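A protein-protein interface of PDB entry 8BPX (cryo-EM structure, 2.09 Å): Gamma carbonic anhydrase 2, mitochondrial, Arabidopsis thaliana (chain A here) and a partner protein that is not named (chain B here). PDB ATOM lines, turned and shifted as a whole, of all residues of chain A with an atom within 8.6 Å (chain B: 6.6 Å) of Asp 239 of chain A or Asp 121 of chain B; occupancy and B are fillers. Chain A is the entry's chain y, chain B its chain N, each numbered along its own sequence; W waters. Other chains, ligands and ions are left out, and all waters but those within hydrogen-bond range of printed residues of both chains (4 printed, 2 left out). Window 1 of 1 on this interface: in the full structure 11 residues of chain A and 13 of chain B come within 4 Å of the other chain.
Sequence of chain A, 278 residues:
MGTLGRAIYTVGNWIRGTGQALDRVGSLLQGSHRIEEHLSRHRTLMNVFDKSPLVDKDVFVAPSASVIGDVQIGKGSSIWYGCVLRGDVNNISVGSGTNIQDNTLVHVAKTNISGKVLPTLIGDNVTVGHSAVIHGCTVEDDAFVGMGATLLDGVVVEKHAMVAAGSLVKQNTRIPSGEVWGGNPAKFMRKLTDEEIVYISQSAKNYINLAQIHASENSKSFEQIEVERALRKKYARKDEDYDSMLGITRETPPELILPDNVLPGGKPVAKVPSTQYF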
ATOM      1  N   LYS A 234      29.604 -19.034  -2.098  1.00  0.00           N
ATOM      2  CA  LYS A 234      29.387 -20.414  -1.671  1.00  0.00           C
ATOM      3  C   LYS A 234      28.160 -20.542  -0.769  1.00  0.00           C
ATOM      4  O   LYS A 234      27.398 -21.508  -0.885  1.00  0.00           O
ATOM      5  CB  LYS A 234      30.638 -20.948  -0.970  1.00  0.00           C
ATOM      6  CG  LYS A 234      30.403 -22.189  -0.123  1.00  0.00           C
ATOM      7  CD  LYS A 234      31.678 -22.626   0.583  1.00  0.00           C
ATOM      8  CE  LYS A 234      31.680 -24.122   0.841  1.00  0.00           C
ATOM      9  NZ  LYS A 234      30.491 -24.540   1.640  1.00  0.00           N
ATOM     10  N   ALA A 236      25.521 -18.415  -0.507  1.00  0.00           N
ATOM     11  CA  ALA A 236      24.363 -17.620  -0.900  1.00  0.00           C
ATOM     12  C   ALA A 236      23.094 -18.461  -0.977  1.00  0.00           C
ATOM     13  O   ALA A 236      21.995 -17.941  -0.761  1.00  0.00           O
ATOM     14  CB  ALA A 236      24.626 -16.936  -2.241  1.00  0.00           C
ATOM     15  N   ARG A 237      23.219 -19.748  -1.286  1.00  0.00           N
ATOM     16  CA  ARG A 237      22.089 -20.662  -1.372  1.00  0.00           C
ATOM     17  C   ARG A 237      22.408 -21.897  -0.534  1.00  0.00           C
ATOM     18  O   ARG A 237      23.495 -22.018   0.037  1.00  0.00           O
ATOM     19  CB  ARG A 237      21.789 -21.040  -2.828  1.00  0.00           C
ATOM     20  CG  ARG A 237      21.370 -19.884  -3.726  1.00  0.00           C
ATOM     21  CD  ARG A 237      20.036 -19.304  -3.309  1.00  0.00           C
ATOM     22  NE  ARG A 237      19.626 -18.213  -4.184  1.00  0.00           N
ATOM     23  CZ  ARG A 237      18.629 -17.378  -3.930  1.00  0.00           C
ATOM     24  NH1 ARG A 237      17.913 -17.471  -2.821  1.00  0.00           N
ATOM     25  NH2 ARG A 237      18.343 -16.424  -4.812  1.00  0.00           N
ATOM     26  N   LYS A 238      21.457 -22.827  -0.451  1.00  0.00           N
ATOM     27  CA  LYS A 238      21.659 -24.012   0.372  1.00  0.00           C
ATOM     28  C   LYS A 238      20.889 -25.194  -0.198  1.00  0.00           C
ATOM     29  O   LYS A 238      19.922 -25.032  -0.947  1.00  0.00           O
ATOM     30  CB  LYS A 238      21.235 -23.763   1.826  1.00  0.00           C
ATOM     31  CG  LYS A 238      20.078 -22.792   1.980  1.00  0.00           C
ATOM     32  CD  LYS A 238      19.795 -22.494   3.446  1.00  0.00           C
ATOM     33  CE  LYS A 238      20.896 -21.654   4.071  1.00  0.00           C
ATOM     34  NZ  LYS A 238      20.510 -21.161   5.423  1.00  0.00           N
ATOM     35  N   ASP A 239      21.362 -26.407   0.154  1.00  0.00           N
ATOM     36  CA  ASP A 239      20.605 -27.655  -0.016  1.00  0.00           C
ATOM     37  C   ASP A 239      20.720 -28.421   1.300  1.00  0.00           C
ATOM     38  O   ASP A 239      21.536 -29.334   1.439  1.00  0.00           O
ATOM     39  CB  ASP A 239      21.127 -28.484  -1.184  1.00  0.00           C
ATOM     40  CG  ASP A 239      20.246 -29.686  -1.504  1.00  0.00           C
ATOM     41  OD1 ASP A 239      19.232 -29.908  -0.807  1.00  0.00           O
ATOM     42  OD2 ASP A 239      20.565 -30.408  -2.471  1.00  0.00           O
ATOM     43  N   GLU A 240      19.865 -28.069   2.260  1.00  0.00           N
ATOM     44  CA  GLU A 240      19.936 -28.700   3.572  1.00  0.00           C
ATOM     45  C   GLU A 240      19.499 -30.156   3.536  1.00  0.00           C
ATOM     46  O   GLU A 240      19.946 -30.945   4.371  1.00  0.00           O
ATOM     47  CB  GLU A 240      19.090 -27.918   4.575  1.00  0.00           C
ATOM     48  CG  GLU A 240      19.510 -26.470   4.728  1.00  0.00           C
ATOM     49  CD  GLU A 240      19.198 -25.917   6.106  1.00  0.00           C
ATOM     50  OE1 GLU A 240      18.546 -24.856   6.187  1.00  0.00           O
ATOM     51  OE2 GLU A 240      19.608 -26.545   7.105  1.00  0.00           O
ATOM     52  N   ASP A 241      18.645 -30.528   2.585  1.00  0.00           N
ATOM     53  CA  ASP A 241      18.235 -31.921   2.465  1.00  0.00           C
ATOM     54  C   ASP A 241      19.403 -32.817   2.061  1.00  0.00           C
ATOM     55  O   ASP A 241      19.600 -33.894   2.637  1.00  0.00           O
ATOM     56  CB  ASP A 241      17.095 -32.032   1.458  1.00  0.00           C
ATOM     57  CG  ASP A 241      16.456 -33.391   1.461  1.00  0.00           C
ATOM     58  OD1 ASP A 241      16.391 -34.019   2.537  1.00  0.00           O
ATOM     59  OD2 ASP A 241      16.028 -33.832   0.380  1.00  0.00           O
ATOM     60  N   TYR A 242      20.202 -32.382   1.084  1.00  0.00           N
ATOM     61  CA  TYR A 242      21.372 -33.166   0.707  1.00  0.00           C
ATOM     62  C   TYR A 242      22.423 -33.165   1.805  1.00  0.00           C
ATOM     63  O   TYR A 242      23.141 -34.155   1.970  1.00  0.00           O
ATOM     64  CB  TYR A 242      21.977 -32.653  -0.596  1.00  0.00           C
ATOM     65  CG  TYR A 242      22.816 -33.690  -1.309  1.00  0.00           C
ATOM     66  CD1 TYR A 242      22.217 -34.750  -1.977  1.00  0.00           C
ATOM     67  CD2 TYR A 242      24.202 -33.615  -1.302  1.00  0.00           C
ATOM     68  CE1 TYR A 242      22.973 -35.699  -2.629  1.00  0.00           C
ATOM     69  CE2 TYR A 242      24.973 -34.564  -1.954  1.00  0.00           C
ATOM     70  CZ  TYR A 242      24.352 -35.604  -2.616  1.00  0.00           C
ATOM     71  OH  TYR A 242      25.102 -36.553  -3.267  1.00  0.00           O
ATOM     72  N   ASP A 243      22.540 -32.065   2.555  1.00  0.00           N
ATOM     73  CA  ASP A 243      23.436 -32.057   3.707  1.00  0.00           C
ATOM     74  C   ASP A 243      22.997 -33.076   4.751  1.00  0.00           C
ATOM     75  O   ASP A 243      23.830 -33.789   5.320  1.00  0.00           O
ATOM     76  CB  ASP A 243      23.501 -30.658   4.321  1.00  0.00           C
ATOM     77  CG  ASP A 243      24.300 -29.687   3.473  1.00  0.00           C
ATOM     78  OD1 ASP A 243      23.707 -28.731   2.937  1.00  0.00           O
ATOM     79  OD2 ASP A 243      25.522 -29.886   3.337  1.00  0.00           O
ATOM     80  N   SER A 244      21.690 -33.159   5.012  1.00  0.00           N
ATOM     81  CA  SER A 244      21.190 -34.158   5.949  1.00  0.00           C
ATOM     82  C   SER A 244      21.460 -35.567   5.436  1.00  0.00           C
ATOM     83  O   SER A 244      21.776 -36.468   6.221  1.00  0.00           O
ATOM     84  CB  SER A 244      19.697 -33.947   6.205  1.00  0.00           C
ATOM     85  OG  SER A 244      18.910 -34.642   5.259  1.00  0.00           O
ATOM     86  N   MET A 245      21.342 -35.778   4.122  1.00  0.00           N
ATOM     87  CA  MET A 245      21.741 -37.067   3.563  1.00  0.00           C
ATOM     88  C   MET A 245      23.221 -37.334   3.813  1.00  0.00           C
ATOM     89  O   MET A 245      23.606 -38.451   4.176  1.00  0.00           O
ATOM     90  CB  MET A 245      21.437 -37.136   2.066  1.00  0.00           C
ATOM     91  CG  MET A 245      21.570 -38.548   1.497  1.00  0.00           C
ATOM     92  SD  MET A 245      21.871 -38.635  -0.281  1.00  0.00           S
ATOM     93  CE  MET A 245      23.584 -38.131  -0.359  1.00  0.00           C
ATOM     94  N   LEU A 246      24.065 -36.316   3.631  1.00  0.00           N
ATOM     95  CA  LEU A 246      25.490 -36.454   3.904  1.00  0.00           C
ATOM     96  C   LEU A 246      25.795 -36.472   5.395  1.00  0.00           C
ATOM     97  O   LEU A 246      26.903 -36.853   5.782  1.00  0.00           O
ATOM     98  CB  LEU A 246      26.269 -35.318   3.235  1.00  0.00           C
ATOM     99  CG  LEU A 246      26.519 -35.405   1.726  1.00  0.00           C
ATOM    100  CD1 LEU A 246      26.876 -34.039   1.151  1.00  0.00           C
ATOM    101  CD2 LEU A 246      27.613 -36.412   1.428  1.00  0.00           C
ATOM    102  N   ILE A 248      25.971 -33.732   7.429  1.00  0.00           N
ATOM    103  CA  ILE A 248      26.819 -32.593   7.757  1.00  0.00           C
ATOM    104  C   ILE A 248      25.936 -31.367   7.922  1.00  0.00           C
ATOM    105  O   ILE A 248      24.795 -31.323   7.460  1.00  0.00           O
ATOM    106  CB  ILE A 248      27.899 -32.324   6.687  1.00  0.00           C
ATOM    107  CG1 ILE A 248      27.245 -31.855   5.384  1.00  0.00           C
ATOM    108  CG2 ILE A 248      28.762 -33.554   6.464  1.00  0.00           C
ATOM    109  CD1 ILE A 248      28.186 -31.127   4.454  1.00  0.00           C
ATOM    110  N   THR A 249      26.488 -30.354   8.584  1.00  0.00           N
ATOM    111  CA  THR A 249      25.783 -29.098   8.805  1.00  0.00           C
ATOM    112  C   THR A 249      26.713 -27.954   8.432  1.00  0.00           C
ATOM    113  O   THR A 249      27.705 -27.703   9.123  1.00  0.00           O
ATOM    114  CB  THR A 249      25.312 -28.970  10.250  1.00  0.00           C
ATOM    115  OG1 THR A 249      24.332 -29.978  10.520  1.00  0.00           O
ATOM    116  CG2 THR A 249      24.694 -27.603  10.480  1.00  0.00           C
ATOM    117  N   ARG A 250      26.393 -27.273   7.339  1.00  0.00           N
ATOM    118  CA  ARG A 250      27.194 -26.150   6.879  1.00  0.00           C
ATOM    119  C   ARG A 250      26.896 -24.929   7.736  1.00  0.00           C
ATOM    120  O   ARG A 250      25.733 -24.568   7.933  1.00  0.00           O
ATOM    121  CB  ARG A 250      26.903 -25.866   5.407  1.00  0.00           C
ATOM    122  CG  ARG A 250      26.964 -27.113   4.540  1.00  0.00           C
ATOM    123  CD  ARG A 250      27.165 -26.778   3.083  1.00  0.00           C
ATOM    124  NE  ARG A 250      27.092 -27.967   2.241  1.00  0.00           N
ATOM    125  CZ  ARG A 250      28.147 -28.658   1.836  1.00  0.00           C
ATOM    126  NH1 ARG A 250      29.374 -28.319   2.195  1.00  0.00           N
ATOM    127  NH2 ARG A 250      27.968 -29.715   1.049  1.00  0.00           N
ATOM    128  N   SER B  40      32.029 -36.380  -3.180  1.00  0.00           N
ATOM    129  CA  SER B  40      30.946 -35.780  -2.410  1.00  0.00           C
ATOM    130  C   SER B  40      31.091 -36.059  -0.916  1.00  0.00           C
ATOM    131  O   SER B  40      30.634 -35.262  -0.091  1.00  0.00           O
ATOM    132  CB  SER B  40      29.597 -36.289  -2.915  1.00  0.00           C
ATOM    133  OG  SER B  40      29.155 -37.400  -2.164  1.00  0.00           O
ATOM    134  N   PRO B  48      31.996 -31.037  -1.487  1.00  0.00           N
ATOM    135  CA  PRO B  48      31.558 -30.141  -2.552  1.00  0.00           C
ATOM    136  C   PRO B  48      30.314 -30.675  -3.231  1.00  0.00           C
ATOM    137  O   PRO B  48      30.154 -31.894  -3.386  1.00  0.00           O
ATOM    138  CB  PRO B  48      32.753 -30.129  -3.514  1.00  0.00           C
ATOM    139  CG  PRO B  48      33.404 -31.451  -3.299  1.00  0.00           C
ATOM    140  CD  PRO B  48      33.234 -31.754  -1.841  1.00  0.00           C
ATOM    141  N   PRO B  49      29.396 -29.800  -3.630  1.00  0.00           N
ATOM    142  CA  PRO B  49      28.332 -30.231  -4.540  1.00  0.00           C
ATOM    143  C   PRO B  49      28.932 -30.627  -5.879  1.00  0.00           C
ATOM    144  O   PRO B  49      29.784 -29.927  -6.426  1.00  0.00           O
ATOM    145  CB  PRO B  49      27.440 -28.990  -4.660  1.00  0.00           C
ATOM    146  CG  PRO B  49      27.774 -28.159  -3.460  1.00  0.00           C
ATOM    147  CD  PRO B  49      29.232 -28.398  -3.216  1.00  0.00           C
ATOM    148  N   LEU B  50      28.487 -31.767  -6.404  1.00  0.00           N
ATOM    149  CA  LEU B  50      29.037 -32.295  -7.646  1.00  0.00           C
ATOM    150  C   LEU B  50      27.992 -32.459  -8.738  1.00  0.00           C
ATOM    151  O   LEU B  50      28.284 -33.077  -9.767  1.00  0.00           O
ATOM    152  CB  LEU B  50      29.745 -33.629  -7.387  1.00  0.00           C
ATOM    153  CG  LEU B  50      30.959 -33.543  -6.463  1.00  0.00           C
ATOM    154  CD1 LEU B  50      31.580 -34.916  -6.250  1.00  0.00           C
ATOM    155  CD2 LEU B  50      31.977 -32.552  -7.011  1.00  0.00           C
ATOM    156  N   ALA B  51      26.789 -31.909  -8.554  1.00  0.00           N
ATOM    157  CA  ALA B  51      25.753 -32.064  -9.566  1.00  0.00           C
ATOM    158  C   ALA B  51      26.168 -31.424 -10.886  1.00  0.00           C
ATOM    159  O   ALA B  51      25.964 -32.011 -11.952  1.00  0.00           O
ATOM    160  CB  ALA B  51      24.432 -31.476  -9.071  1.00  0.00           C
ATOM    161  N   SER B  52      26.763 -30.229 -10.839  1.00  0.00           N
ATOM    162  CA  SER B  52      27.160 -29.558 -12.073  1.00  0.00           C
ATOM    163  C   SER B  52      28.410 -30.183 -12.691  1.00  0.00           C
ATOM    164  O   SER B  52      28.491 -30.322 -13.916  1.00  0.00           O
ATOM    165  CB  SER B  52      27.368 -28.063 -11.821  1.00  0.00           C
ATOM    166  OG  SER B  52      28.503 -27.818 -11.012  1.00  0.00           O
ATOM    167  N   PHE B 115      20.808 -26.603 -10.925  1.00  0.00           N
ATOM    168  CA  PHE B 115      21.727 -27.210  -9.967  1.00  0.00           C
ATOM    169  C   PHE B 115      22.309 -26.169  -9.018  1.00  0.00           C
ATOM    170  O   PHE B 115      22.306 -26.359  -7.798  1.00  0.00           O
ATOM    171  CB  PHE B 115      22.855 -27.945 -10.694  1.00  0.00           C
ATOM    172  CG  PHE B 115      22.429 -29.226 -11.342  1.00  0.00           C
ATOM    173  CD1 PHE B 115      21.324 -29.920 -10.883  1.00  0.00           C
ATOM    174  CD2 PHE B 115      23.149 -29.748 -12.404  1.00  0.00           C
ATOM    175  CE1 PHE B 115      20.936 -31.102 -11.480  1.00  0.00           C
ATOM    176  CE2 PHE B 115      22.766 -30.928 -13.003  1.00  0.00           C
ATOM    177  CZ  PHE B 115      21.661 -31.607 -12.540  1.00  0.00           C
ATOM    178  N   ASP B 116      22.810 -25.056  -9.555  1.00  0.00           N
ATOM    179  CA  ASP B 116      23.570 -24.153  -8.693  1.00  0.00           C
ATOM    180  C   ASP B 116      22.704 -23.157  -7.932  1.00  0.00           C
ATOM    181  O   ASP B 116      23.041 -22.810  -6.795  1.00  0.00           O
ATOM    182  CB  ASP B 116      24.636 -23.393  -9.488  1.00  0.00           C
ATOM    183  CG  ASP B 116      24.099 -22.760 -10.739  1.00  0.00           C
ATOM    184  OD1 ASP B 116      22.908 -22.401 -10.764  1.00  0.00           O
ATOM    185  OD2 ASP B 116      24.879 -22.609 -11.700  1.00  0.00           O
ATOM    186  N   GLU B 118      19.095 -23.274  -7.217  1.00  0.00           N
ATOM    187  CA  GLU B 118      18.303 -23.989  -6.228  1.00  0.00           C
ATOM    188  C   GLU B 118      19.202 -24.624  -5.181  1.00  0.00           C
ATOM    189  O   GLU B 118      18.794 -24.795  -4.028  1.00  0.00           O
ATOM    190  CB  GLU B 118      17.449 -25.053  -6.916  1.00  0.00           C
ATOM    191  CG  GLU B 118      16.459 -25.758  -6.014  1.00  0.00           C
ATOM    192  CD  GLU B 118      15.074 -25.159  -6.109  1.00  0.00           C
ATOM    193  OE1 GLU B 118      14.832 -24.373  -7.049  1.00  0.00           O
ATOM    194  OE2 GLU B 118      14.224 -25.471  -5.248  1.00  0.00           O
ATOM    195  N   ARG B 119      20.449 -24.907  -5.555  1.00  0.00           N
ATOM    196  CA  ARG B 119      21.297 -25.867  -4.864  1.00  0.00           C
ATOM    197  C   ARG B 119      20.558 -27.197  -4.722  1.00  0.00           C
ATOM    198  O   ARG B 119      20.024 -27.557  -3.681  1.00  0.00           O
ATOM    199  CB  ARG B 119      21.824 -25.326  -3.537  1.00  0.00           C
ATOM    200  CG  ARG B 119      22.773 -24.172  -3.755  1.00  0.00           C
ATOM    201  CD  ARG B 119      24.235 -24.608  -3.796  1.00  0.00           C
ATOM    202  NE  ARG B 119      24.534 -25.733  -2.919  1.00  0.00           N
ATOM    203  CZ  ARG B 119      24.862 -25.614  -1.641  1.00  0.00           C
ATOM    204  NH1 ARG B 119      24.895 -24.433  -1.044  1.00  0.00           N
ATOM    205  NH2 ARG B 119      25.169 -26.703  -0.944  1.00  0.00           N
ATOM    206  N   PHE B 120      20.423 -27.832  -5.872  1.00  0.00           N
ATOM    207  CA  PHE B 120      20.194 -29.267  -5.968  1.00  0.00           C
ATOM    208  C   PHE B 120      21.571 -29.898  -6.162  1.00  0.00           C
ATOM    209  O   PHE B 120      22.104 -29.911  -7.272  1.00  0.00           O
ATOM    210  CB  PHE B 120      19.242 -29.570  -7.121  1.00  0.00           C
ATOM    211  CG  PHE B 120      18.772 -30.989  -7.171  1.00  0.00           C
ATOM    212  CD1 PHE B 120      19.545 -31.967  -7.776  1.00  0.00           C
ATOM    213  CD2 PHE B 120      17.552 -31.345  -6.626  1.00  0.00           C
ATOM    214  CE1 PHE B 120      19.111 -33.275  -7.829  1.00  0.00           C
ATOM    215  CE2 PHE B 120      17.114 -32.650  -6.676  1.00  0.00           C
ATOM    216  CZ  PHE B 120      17.894 -33.616  -7.280  1.00  0.00           C
ATOM    217  N   ASP B 121      22.167 -30.397  -5.076  1.00  0.00           N
ATOM    218  CA  ASP B 121      23.539 -30.895  -5.134  1.00  0.00           C
ATOM    219  C   ASP B 121      23.649 -32.372  -5.491  1.00  0.00           C
ATOM    220  O   ASP B 121      24.769 -32.863  -5.648  1.00  0.00           O
ATOM    221  CB  ASP B 121      24.281 -30.669  -3.806  1.00  0.00           C
ATOM    222  CG  ASP B 121      24.143 -29.259  -3.267  1.00  0.00           C
ATOM    223  OD1 ASP B 121      24.386 -28.286  -4.008  1.00  0.00           O
ATOM    224  OD2 ASP B 121      23.876 -29.130  -2.063  1.00  0.00           O
ATOM    225  N   ALA B 122      22.536 -33.089  -5.619  1.00  0.00           N
ATOM    226  CA  ALA B 122      22.586 -34.536  -5.820  1.00  0.00           C
ATOM    227  C   ALA B 122      23.102 -34.858  -7.218  1.00  0.00           C
ATOM    228  O   ALA B 122      22.404 -34.637  -8.211  1.00  0.00           O
ATOM    229  CB  ALA B 122      21.209 -35.151  -5.593  1.00  0.00           C
ATOM    230  N   PHE B 123      24.329 -35.379  -7.301  1.00  0.00           N
ATOM    231  CA  PHE B 123      24.850 -35.846  -8.581  1.00  0.00           C
ATOM    232  C   PHE B 123      24.169 -37.128  -9.044  1.00  0.00           C
ATOM    233  O   PHE B 123      24.226 -37.449 -10.235  1.00  0.00           O
ATOM    234  CB  PHE B 123      26.360 -36.078  -8.491  1.00  0.00           C
ATOM    235  CG  PHE B 123      26.735 -37.323  -7.742  1.00  0.00           C
ATOM    236  CD1 PHE B 123      26.880 -38.534  -8.403  1.00  0.00           C
ATOM    237  CD2 PHE B 123      26.937 -37.284  -6.374  1.00  0.00           C
ATOM    238  CE1 PHE B 123      27.217 -39.679  -7.713  1.00  0.00           C
ATOM    239  CE2 PHE B 123      27.274 -38.426  -5.680  1.00  0.00           C
ATOM    240  CZ  PHE B 123      27.412 -39.624  -6.347  1.00  0.00           C
ATOM    241  N   GLU B 124      23.553 -37.874  -8.125  1.00  0.00           N
ATOM    242  CA  GLU B 124      22.879 -39.115  -8.496  1.00  0.00           C
ATOM    243  C   GLU B 124      21.768 -38.864  -9.505  1.00  0.00           C
ATOM    244  O   GLU B 124      21.394 -39.769 -10.255  1.00  0.00           O
ATOM    245  CB  GLU B 124      22.325 -39.801  -7.247  1.00  0.00           C
ATOM    246  CG  GLU B 124      23.395 -40.378  -6.328  1.00  0.00           C
ATOM    247  CD  GLU B 124      23.859 -39.398  -5.256  1.00  0.00           C
ATOM    248  OE1 GLU B 124      23.756 -38.173  -5.469  1.00  0.00           O
ATOM    249  OE2 GLU B 124      24.335 -39.860  -4.200  1.00  0.00           O
ATOM    250  N   LYS B 166      13.013 -34.358  -5.063  1.00  0.00           N
ATOM    251  CA  LYS B 166      12.800 -33.367  -3.969  1.00  0.00           C
ATOM    252  C   LYS B 166      12.062 -34.166  -2.898  1.00  0.00           C
ATOM    253  O   LYS B 166      10.826 -34.086  -2.837  1.00  0.00           O
ATOM    254  CB  LYS B 166      12.080 -32.114  -4.480  1.00  0.00           C
ATOM    255  CG  LYS B 166      12.878 -31.293  -5.486  1.00  0.00           C
ATOM    256  CD  LYS B 166      13.072 -29.847  -5.080  1.00  0.00           C
ATOM    257  CE  LYS B 166      13.924 -29.681  -3.841  1.00  0.00           C
ATOM    258  NZ  LYS B 166      14.132 -28.251  -3.507  1.00  0.00           N
HETATM  259  O   HOH W   1      25.104 -30.678  -0.371  1.00  0.00           O
HETATM  260  O   HOH W   2      23.466 -26.510   1.474  1.00  0.00           O
HETATM  261  O   HOH W   3      27.632 -31.566  -1.487  1.00  0.00           O
HETATM  262  O   HOH W   4      19.559 -32.705  -4.321  1.00  0.00           O
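Of chain B, only Arg 119 (2.9 Å), Phe 120 (3.7 Å) and Asp 121 (3.0 Å) come within 4 Å of Asp 239 of chain A.
Asp 241 of chain A touches none of the printed residues of chain B.
Asp 243 of chain A touches none of the printed residues of chain B.
Of the printed residues of chain A, Glu 118 of chain B touches Lys 238.
Of the printed residues of chain A, Asp 121 of chain B touches Asp 239 (3.0 Å) and Tyr 242 (3.9 Å).
Ala 122 of chain B touches one residue of chain A.
Printed residues of chain A within 4 Å of Phe 123 of chain B: Tyr 242 (3.7 Å).
The nearest residue of chain A that does not touch Asp 121 of chain B is Asp 243 of chain A (5.0 Å).
Of the 15 printed residues of chain A, 7 touch a printed residue of chain B.
Hydrophobic or aromatic side chains of chain A within 4 Å of the printed part of chain B: Tyr 242 and Leu 246.
Printed residues of chain B that touch a printed residue of chain A: Ser 40, Glu 118, Arg 119, Phe 120, Asp 121, Ala 122, Phe 123 and Glu 124.
Among the printed residues, 13 pairs touch across the chains.
Among the printed residues, no Asp or Glu carboxylate lies within 4 Å of a Lys or Arg side-chain nitrogen of the other chain.
O of Arg 119 of chain B lies close to OD2 of Asp 239 of chain A (3.1 Å).
The guanidinium group (NH1) of Arg 119 of chain B is in hydrogen-bond range of the backbone carbonyl oxygen (O) of Arg 237 of chain A.
OH of Tyr 242 of chain A is in hydrogen-bond range of OE1 of Glu 124 of chain B, at 3.0 Å.
The backbone carbonyl oxygen (O) of Glu 118 of chain B sits close to the backbone carbonyl oxygen (O) of Lys 238 of chain A, at 3.3 Å.
The backbone NH (N) of Asp 121 of chain B sits at hydrogen-bond distance from the side-chain carboxylate (OD2) of Asp 239 of chain A (3.1 Å).
Water W2 lies within hydrogen-bond range of N of Asp 239 of chain A (2.5 Å), OD1 of Asp 243 of chain A (2.7 Å) and NH2 of Arg 119 of chain B (3.0 Å).
Water W1 bridges OD2 of Asp 121 of chain B and NH2 of Arg 250 of chain A.
Water W4 lies within hydrogen-bond range of OD2 of Asp 239 of chain A (3.1 Å) and N of Ala 122 of chain B (3.3 Å).
Water W3 lies within hydrogen-bond range of the guanidinium group of Arg 250 of chain A (3.2 Å) and the backbone carbonyl oxygen of Pro 48 of chain B (3.2 Å).
Among the printed residues, merely in contact across the chains: Lys 234 of chain A with Arg 119 of chain B (3.9 Å), Lys 238 of chain A with Arg 119 of chain B (3.2 Å), Asp 239 of chain A with Phe 120 of chain B (3.7 Å), Tyr 242 of chain A with Asp 121 of chain B (3.9 Å), Tyr 242 of chain A with Ala 122 of chain B (3.4 Å), Tyr 242 of chain A with Phe 123 of chain B (3.7 Å), Leu 246 of chain A with Ser 40 of chain B (3.6 Å) and Arg 250 of chain A with Arg 119 of chain B (3.9 Å).
The backbone NH (N) of Asp 241 of chain A sits close to the side-chain carboxylate (OD1) of Asp 239 of chain A, at 3.5 Å.
The side-chain carboxylate (OD1) of Asp 239 of chain A sits at hydrogen-bond distance from the backbone NH (N) of Tyr 242 of chain A (3.3 Å).
The side-chain carboxylate of Asp 121 of chain B lies within salt-bridge range of the guanidinium group of Arg 119 of chain B (2.8 Å).
The side-chain carboxylate (OE2) of Glu 118 of chain B is in salt-bridge range of the side-chain amino group (NZ) of Lys 166 of chain B (3.3 Å).
O of Asp 239 of chain A sits close to OD1 of Asp 243 of chain A (2.7 Å).
O of Phe 115 of chain B is in hydrogen-bond range of N of Phe 120 of chain B (3.1 Å).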
